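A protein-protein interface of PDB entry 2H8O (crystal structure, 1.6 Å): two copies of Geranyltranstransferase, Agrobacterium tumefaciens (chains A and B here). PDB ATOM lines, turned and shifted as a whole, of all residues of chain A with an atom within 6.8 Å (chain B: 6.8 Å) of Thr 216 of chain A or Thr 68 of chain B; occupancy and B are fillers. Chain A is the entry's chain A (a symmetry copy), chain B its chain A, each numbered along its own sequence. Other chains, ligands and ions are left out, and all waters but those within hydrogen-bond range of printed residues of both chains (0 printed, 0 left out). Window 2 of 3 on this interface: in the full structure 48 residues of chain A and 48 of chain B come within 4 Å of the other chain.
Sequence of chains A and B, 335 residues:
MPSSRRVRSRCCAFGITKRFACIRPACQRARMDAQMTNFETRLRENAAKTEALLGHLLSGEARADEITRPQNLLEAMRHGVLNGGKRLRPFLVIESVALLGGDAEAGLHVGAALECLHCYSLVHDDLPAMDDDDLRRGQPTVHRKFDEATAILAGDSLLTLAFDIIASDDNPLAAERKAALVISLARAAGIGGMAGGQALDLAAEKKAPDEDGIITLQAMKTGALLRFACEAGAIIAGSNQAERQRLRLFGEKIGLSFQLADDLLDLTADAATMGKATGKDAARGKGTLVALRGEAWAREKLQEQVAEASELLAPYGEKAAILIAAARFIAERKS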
ATOM      1  N   GLY A 190     -29.085  -3.664 -17.520  1.00  0.00           N
ATOM      2  CA  GLY A 190     -29.340  -3.905 -18.933  1.00  0.00           C
ATOM      3  C   GLY A 190     -28.464  -4.964 -19.573  1.00  0.00           C
ATOM      4  O   GLY A 190     -28.069  -5.937 -18.934  1.00  0.00           O
ATOM      5  N   ILE A 191     -28.223  -4.773 -20.861  1.00  0.00           N
ATOM      6  CA  ILE A 191     -27.482  -5.729 -21.713  1.00  0.00           C
ATOM      7  C   ILE A 191     -26.139  -6.125 -21.092  1.00  0.00           C
ATOM      8  O   ILE A 191     -25.708  -7.296 -21.208  1.00  0.00           O
ATOM      9  CB  ILE A 191     -27.267  -5.174 -23.163  1.00  0.00           C
ATOM     10  CG1 ILE A 191     -26.460  -6.156 -24.037  1.00  0.00           C
ATOM     11  CG2 ILE A 191     -26.584  -3.772 -23.145  1.00  0.00           C
ATOM     12  CD1 ILE A 191     -27.134  -7.473 -24.221  1.00  0.00           C
ATOM     13  N   GLY A 192     -25.466  -5.164 -20.476  1.00  0.00           N
ATOM     14  CA  GLY A 192     -24.152  -5.438 -19.841  1.00  0.00           C
ATOM     15  C   GLY A 192     -24.212  -5.716 -18.348  1.00  0.00           C
ATOM     16  O   GLY A 192     -23.198  -5.687 -17.662  1.00  0.00           O
ATOM     17  N   GLY A 193     -25.417  -5.940 -17.845  1.00  0.00           N
ATOM     18  CA  GLY A 193     -25.678  -6.200 -16.439  1.00  0.00           C
ATOM     19  C   GLY A 193     -26.741  -7.288 -16.307  1.00  0.00           C
ATOM     20  O   GLY A 193     -26.704  -8.296 -17.013  1.00  0.00           O
ATOM     21  N   GLY A 196     -28.548  -9.029 -19.350  1.00  0.00           N
ATOM     22  CA  GLY A 196     -27.546  -9.826 -20.060  1.00  0.00           C
ATOM     23  C   GLY A 196     -27.179 -11.080 -19.305  1.00  0.00           C
ATOM     24  O   GLY A 196     -26.973 -12.152 -19.900  1.00  0.00           O
ATOM     25  N   GLY A 197     -27.056 -10.956 -17.988  1.00  0.00           N
ATOM     26  CA  GLY A 197     -26.787 -12.124 -17.141  1.00  0.00           C
ATOM     27  C   GLY A 197     -27.872 -13.168 -17.216  1.00  0.00           C
ATOM     28  O   GLY A 197     -27.592 -14.365 -17.228  1.00  0.00           O
ATOM     29  N   LEU A 200     -27.360 -14.983 -20.355  1.00  0.00           N
ATOM     30  CA  LEU A 200     -26.243 -15.931 -20.250  1.00  0.00           C
ATOM     31  C   LEU A 200     -26.645 -17.144 -19.424  1.00  0.00           C
ATOM     32  O   LEU A 200     -26.217 -18.275 -19.709  1.00  0.00           O
ATOM     33  CB  LEU A 200     -24.997 -15.247 -19.678  1.00  0.00           C
ATOM     34  CG  LEU A 200     -24.319 -14.264 -20.636  1.00  0.00           C
ATOM     35  CD1 LEU A 200     -23.210 -13.513 -19.927  1.00  0.00           C
ATOM     36  CD2 LEU A 200     -23.775 -14.988 -21.852  1.00  0.00           C
ATOM     37  N   GLU A 211     -15.623 -21.998 -15.953  1.00  0.00           N
ATOM     38  CA  GLU A 211     -15.573 -21.218 -14.734  1.00  0.00           C
ATOM     39  C   GLU A 211     -15.639 -19.704 -15.015  1.00  0.00           C
ATOM     40  O   GLU A 211     -16.372 -18.975 -14.369  1.00  0.00           O
ATOM     41  CB  GLU A 211     -14.323 -21.569 -13.936  1.00  0.00           C
ATOM     42  CG  GLU A 211     -14.355 -21.053 -12.537  1.00  0.00           C
ATOM     43  CD  GLU A 211     -13.214 -21.580 -11.689  1.00  0.00           C
ATOM     44  OE1 GLU A 211     -12.635 -22.644 -12.004  1.00  0.00           O
ATOM     45  OE2 GLU A 211     -12.913 -20.907 -10.691  1.00  0.00           O
ATOM     46  N   ASP A 212     -14.867 -19.247 -15.987  1.00  0.00           N
ATOM     47  CA  ASP A 212     -14.880 -17.835 -16.352  1.00  0.00           C
ATOM     48  C   ASP A 212     -16.300 -17.408 -16.771  1.00  0.00           C
ATOM     49  O   ASP A 212     -16.765 -16.300 -16.445  1.00  0.00           O
ATOM     50  CB  ASP A 212     -13.872 -17.592 -17.471  1.00  0.00           C
ATOM     51  CG  ASP A 212     -13.737 -16.121 -17.822  1.00  0.00           C
ATOM     52  OD1 ASP A 212     -13.225 -15.368 -16.967  1.00  0.00           O
ATOM     53  OD2 ASP A 212     -14.139 -15.735 -18.944  1.00  0.00           O
ATOM     54  N   GLY A 213     -16.994 -18.283 -17.485  1.00  0.00           N
ATOM     55  CA  GLY A 213     -18.361 -17.984 -17.906  1.00  0.00           C
ATOM     56  C   GLY A 213     -19.340 -17.866 -16.756  1.00  0.00           C
ATOM     57  O   GLY A 213     -20.238 -16.998 -16.764  1.00  0.00           O
ATOM     58  N   ILE A 214     -19.186 -18.746 -15.766  1.00  0.00           N
ATOM     59  CA  ILE A 214     -20.027 -18.737 -14.578  1.00  0.00           C
ATOM     60  C   ILE A 214     -19.806 -17.447 -13.788  1.00  0.00           C
ATOM     61  O   ILE A 214     -20.745 -16.773 -13.379  1.00  0.00           O
ATOM     62  CB  ILE A 214     -19.763 -19.965 -13.674  1.00  0.00           C
ATOM     63  CG1 ILE A 214     -20.179 -21.254 -14.390  1.00  0.00           C
ATOM     64  CG2 ILE A 214     -20.513 -19.841 -12.347  1.00  0.00           C
ATOM     65  CD1 ILE A 214     -19.707 -22.523 -13.685  1.00  0.00           C
ATOM     66  N   ILE A 215     -18.539 -17.083 -13.591  1.00  0.00           N
ATOM     67  CA  ILE A 215     -18.221 -15.885 -12.824  1.00  0.00           C
ATOM     68  C   ILE A 215     -18.861 -14.664 -13.493  1.00  0.00           C
ATOM     69  O   ILE A 215     -19.481 -13.802 -12.845  1.00  0.00           O
ATOM     70  CB  ILE A 215     -16.671 -15.720 -12.703  1.00  0.00           C
ATOM     71  CG1 ILE A 215     -16.122 -16.865 -11.835  1.00  0.00           C
ATOM     72  CG2 ILE A 215     -16.298 -14.334 -12.170  1.00  0.00           C
ATOM     73  CD1 ILE A 215     -14.591 -17.025 -11.823  1.00  0.00           C
ATOM     74  N   THR A 216     -18.747 -14.619 -14.812  1.00  0.00           N
ATOM     75  CA  THR A 216     -19.311 -13.504 -15.586  1.00  0.00           C
ATOM     76  C   THR A 216     -20.830 -13.454 -15.486  1.00  0.00           C
ATOM     77  O   THR A 216     -21.397 -12.389 -15.190  1.00  0.00           O
ATOM     78  CB  THR A 216     -18.854 -13.577 -17.052  1.00  0.00           C
ATOM     79  OG1 THR A 216     -17.431 -13.377 -17.086  1.00  0.00           O
ATOM     80  CG2 THR A 216     -19.564 -12.524 -17.946  1.00  0.00           C
ATOM     81  N   LEU A 217     -21.512 -14.571 -15.723  1.00  0.00           N
ATOM     82  CA  LEU A 217     -22.974 -14.523 -15.698  1.00  0.00           C
ATOM     83  C   LEU A 217     -23.497 -14.212 -14.293  1.00  0.00           C
ATOM     84  O   LEU A 217     -24.510 -13.503 -14.144  1.00  0.00           O
ATOM     85  CB  LEU A 217     -23.609 -15.775 -16.291  1.00  0.00           C
ATOM     86  CG  LEU A 217     -23.652 -17.086 -15.524  1.00  0.00           C
ATOM     87  CD1 LEU A 217     -24.821 -17.073 -14.533  1.00  0.00           C
ATOM     88  CD2 LEU A 217     -23.759 -18.281 -16.520  1.00  0.00           C
ATOM     89  N   GLN A 218     -22.809 -14.713 -13.266  1.00  0.00           N
ATOM     90  CA  GLN A 218     -23.177 -14.396 -11.880  1.00  0.00           C
ATOM     91  C   GLN A 218     -22.971 -12.915 -11.530  1.00  0.00           C
ATOM     92  O   GLN A 218     -23.827 -12.293 -10.913  1.00  0.00           O
ATOM     93  CB  GLN A 218     -22.384 -15.272 -10.913  1.00  0.00           C
ATOM     94  CG  GLN A 218     -22.785 -16.727 -10.961  1.00  0.00           C
ATOM     95  CD  GLN A 218     -22.017 -17.583  -9.976  1.00  0.00           C
ATOM     96  OE1 GLN A 218     -20.965 -17.188  -9.448  1.00  0.00           O
ATOM     97  NE2 GLN A 218     -22.543 -18.769  -9.722  1.00  0.00           N
ATOM     98  N   ALA A 219     -21.826 -12.355 -11.935  1.00  0.00           N
ATOM     99  CA  ALA A 219     -21.548 -10.934 -11.720  1.00  0.00           C
ATOM    100  C   ALA A 219     -22.625 -10.060 -12.342  1.00  0.00           C
ATOM    101  O   ALA A 219     -22.950  -9.002 -11.808  1.00  0.00           O
ATOM    102  CB  ALA A 219     -20.173 -10.558 -12.281  1.00  0.00           C
ATOM    103  N   MET A 220     -23.195 -10.521 -13.459  1.00  0.00           N
ATOM    104  CA  MET A 220     -24.235  -9.782 -14.173  1.00  0.00           C
ATOM    105  C   MET A 220     -25.621 -10.036 -13.565  1.00  0.00           C
ATOM    106  O   MET A 220     -26.318  -9.088 -13.192  1.00  0.00           O
ATOM    107  CB  MET A 220     -24.208 -10.133 -15.677  1.00  0.00           C
ATOM    108  CG  MET A 220     -22.905  -9.739 -16.382  1.00  0.00           C
ATOM    109  SD  MET A 220     -22.709 -10.363 -18.103  1.00  0.00           S
ATOM    110  CE  MET A 220     -23.885  -9.318 -18.992  1.00  0.00           C
ATOM    111  N   LYS A 221     -25.985 -11.304 -13.454  1.00  0.00           N
ATOM    112  CA  LYS A 221     -27.347 -11.695 -13.095  1.00  0.00           C
ATOM    113  C   LYS A 221     -27.729 -11.266 -11.693  1.00  0.00           C
ATOM    114  O   LYS A 221     -28.865 -10.812 -11.446  1.00  0.00           O
ATOM    115  CB  LYS A 221     -27.529 -13.189 -13.188  1.00  0.00           C
ATOM    116  CG  LYS A 221     -28.986 -13.607 -13.015  1.00  0.00           C
ATOM    117  CD  LYS A 221     -29.160 -15.084 -13.364  1.00  0.00           C
ATOM    118  CE  LYS A 221     -30.595 -15.614 -13.118  1.00  0.00           C
ATOM    119  NZ  LYS A 221     -31.450 -14.763 -12.275  1.00  0.00           N
ATOM    120  N   GLY B  60     -21.030  -4.232 -30.161  1.00  0.00           N
ATOM    121  CA  GLY B  60     -20.742  -5.329 -29.265  1.00  0.00           C
ATOM    122  C   GLY B  60     -19.783  -5.026 -28.134  1.00  0.00           C
ATOM    123  O   GLY B  60     -19.621  -5.837 -27.230  1.00  0.00           O
ATOM    124  N   GLU B  61     -19.116  -3.886 -28.188  1.00  0.00           N
ATOM    125  CA  GLU B  61     -18.121  -3.473 -27.184  1.00  0.00           C
ATOM    126  C   GLU B  61     -18.813  -3.094 -25.887  1.00  0.00           C
ATOM    127  O   GLU B  61     -19.761  -2.299 -25.923  1.00  0.00           O
ATOM    128  CB  GLU B  61     -17.319  -2.257 -27.693  1.00  0.00           C
ATOM    129  CG  GLU B  61     -18.082  -1.396 -28.724  1.00  0.00           C
ATOM    130  CD  GLU B  61     -17.591   0.029 -28.862  1.00  0.00           C
ATOM    131  OE1 GLU B  61     -16.410   0.306 -28.552  1.00  0.00           O
ATOM    132  OE2 GLU B  61     -18.402   0.879 -29.308  1.00  0.00           O
ATOM    133  N   ALA B  62     -18.343  -3.622 -24.765  1.00  0.00           N
ATOM    134  CA  ALA B  62     -18.874  -3.240 -23.466  1.00  0.00           C
ATOM    135  C   ALA B  62     -18.487  -1.796 -23.172  1.00  0.00           C
ATOM    136  O   ALA B  62     -17.368  -1.369 -23.452  1.00  0.00           O
ATOM    137  CB  ALA B  62     -18.359  -4.160 -22.382  1.00  0.00           C
ATOM    138  N   GLU B  66     -20.369  -1.814 -17.809  1.00  0.00           N
ATOM    139  CA  GLU B  66     -20.907  -3.049 -18.336  1.00  0.00           C
ATOM    140  C   GLU B  66     -19.850  -4.123 -18.251  1.00  0.00           C
ATOM    141  O   GLU B  66     -18.650  -3.859 -18.476  1.00  0.00           O
ATOM    142  CB  GLU B  66     -21.291  -2.884 -19.809  1.00  0.00           C
ATOM    143  CG  GLU B  66     -22.430  -1.894 -20.054  1.00  0.00           C
ATOM    144  CD  GLU B  66     -22.786  -1.714 -21.527  1.00  0.00           C
ATOM    145  OE1 GLU B  66     -22.023  -2.189 -22.402  1.00  0.00           O
ATOM    146  OE2 GLU B  66     -23.850  -1.112 -21.819  1.00  0.00           O
ATOM    147  N   ILE B  67     -20.280  -5.346 -17.990  1.00  0.00           N
ATOM    148  CA  ILE B  67     -19.350  -6.439 -17.839  1.00  0.00           C
ATOM    149  C   ILE B  67     -19.007  -7.021 -19.216  1.00  0.00           C
ATOM    150  O   ILE B  67     -17.834  -7.033 -19.637  1.00  0.00           O
ATOM    151  CB  ILE B  67     -19.903  -7.459 -16.848  1.00  0.00           C
ATOM    152  CG1 ILE B  67     -19.963  -6.799 -15.458  1.00  0.00           C
ATOM    153  CG2 ILE B  67     -19.036  -8.689 -16.790  1.00  0.00           C
ATOM    154  CD1 ILE B  67     -20.859  -7.482 -14.493  1.00  0.00           C
ATOM    155  N   THR B  68     -20.023  -7.477 -19.939  1.00  0.00           N
ATOM    156  CA  THR B  68     -19.876  -7.867 -21.347  1.00  0.00           C
ATOM    157  C   THR B  68     -21.246  -7.749 -21.989  1.00  0.00           C
ATOM    158  O   THR B  68     -22.227  -7.683 -21.264  1.00  0.00           O
ATOM    159  CB  THR B  68     -19.371  -9.301 -21.491  1.00  0.00           C
ATOM    160  OG1 THR B  68     -18.910  -9.531 -22.846  1.00  0.00           O
ATOM    161  CG2 THR B  68     -20.441 -10.295 -21.133  1.00  0.00           C
ATOM    162  N   ARG B  69     -21.314  -7.684 -23.324  1.00  0.00           N
ATOM    163  CA  ARG B  69     -22.603  -7.677 -24.038  1.00  0.00           C
ATOM    164  C   ARG B  69     -22.827  -9.023 -24.719  1.00  0.00           C
ATOM    165  O   ARG B  69     -22.166  -9.322 -25.730  1.00  0.00           O
ATOM    166  CB  ARG B  69     -22.638  -6.542 -25.060  1.00  0.00           C
ATOM    167  CG  ARG B  69     -22.641  -5.163 -24.429  1.00  0.00           C
ATOM    168  CD  ARG B  69     -22.756  -4.051 -25.471  1.00  0.00           C
ATOM    169  NE  ARG B  69     -23.143  -2.808 -24.827  1.00  0.00           N
ATOM    170  CZ  ARG B  69     -23.768  -1.791 -25.425  1.00  0.00           C
ATOM    171  NH1 ARG B  69     -24.069  -1.814 -26.717  1.00  0.00           N
ATOM    172  NH2 ARG B  69     -24.109  -0.735 -24.689  1.00  0.00           N
ATOM    173  N   PRO B  70     -23.712  -9.868 -24.169  1.00  0.00           N
ATOM    174  CA  PRO B  70     -23.919 -11.175 -24.802  1.00  0.00           C
ATOM    175  C   PRO B  70     -24.419 -11.051 -26.213  1.00  0.00           C
ATOM    176  O   PRO B  70     -25.356 -10.305 -26.490  1.00  0.00           O
ATOM    177  CB  PRO B  70     -24.950 -11.865 -23.909  1.00  0.00           C
ATOM    178  CG  PRO B  70     -24.848 -11.170 -22.601  1.00  0.00           C
ATOM    179  CD  PRO B  70     -24.494  -9.746 -22.927  1.00  0.00           C
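The backbone carbonyl oxygen of Gly 192 of chain A is in hydrogen-bond range of the backbone NH of Ile 67 of chain B (3.0 Å).
The side-chain carboxylate of Glu 66 of chain B lies within salt-bridge range of the guanidinium group of Arg 69 of chain B (2.7 Å).
The backbone NH of Gly 196 of chain A lies within hydrogen-bond range of the backbone carbonyl oxygen of Gly 190 of chain A, at 3.2 Å.
The backbone carbonyl oxygen (O) of Asp 212 of chain A sits at hydrogen-bond distance from the side-chain hydroxyl (OG1) of Thr 216 of chain A, at 3.1 Å.
O of Thr 68 of chain B touches O of Ile 191 of chain A, at 3.5 Å.
Ile 191 of chain A touches Arg 69 of chain B.
Ile 191 of chain A touches Pro 70 of chain B (O to CD, 3.2 Å).
O of Gly 192 of chain A touches CA of Glu 66 of chain B, 3.6 Å away.
Thr 68 of chain B touches Gly 192 of chain A.
CG of Pro 70 of chain B touches O of Gly 196 of chain A, 3.6 Å away.
CG2 of Thr 216 of chain A touches CG2 of Thr 68 of chain B, 3.99 Å away.
O of Ala 219 of chain A touches CD1 of Ile 67 of chain B (3.7 Å).
CG of Met 220 of chain A touches CD1 of Ile 67 of chain B, 3.6 Å away.
Thr 68 of chain B touches Met 220 of chain A (O to CE, 3.3 Å).
Of the printed residues of chain B, Leu 200 of chain A touches Pro 70 (3.7 Å).
Of the printed residues of chain B, Thr 216 of chain A touches Thr 68.
Printed residues of chain A within 4 Å of Arg 69 of chain B: Ile 191.
The nearest printed residue of chain B that does not touch Thr 216 of chain A is Ile 67 of chain B (4.04 Å).
The nearest printed residue of chain A that does not touch Thr 68 of chain B is Leu 200 of chain A (4.4 Å).
The nearest printed residue of chain B that does not touch Ala 219 of chain A is Thr 68 of chain B (8.3 Å).
Hydrophobic or aromatic side chains of chain B within 4 Å of the printed part of chain A: Ile 67 and Pro 70.
Of the 18 printed residues of chain A, 7 touch a printed residue of chain B.
Among the printed residues, no Asp or Glu carboxylate lies within 4 Å of a Lys or Arg side-chain nitrogen of the other chain.
No position is printed for both chains.
Of the 12 pairs that touch across the chains among the printed residues, none has its exchanged pair printed and touching as well.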
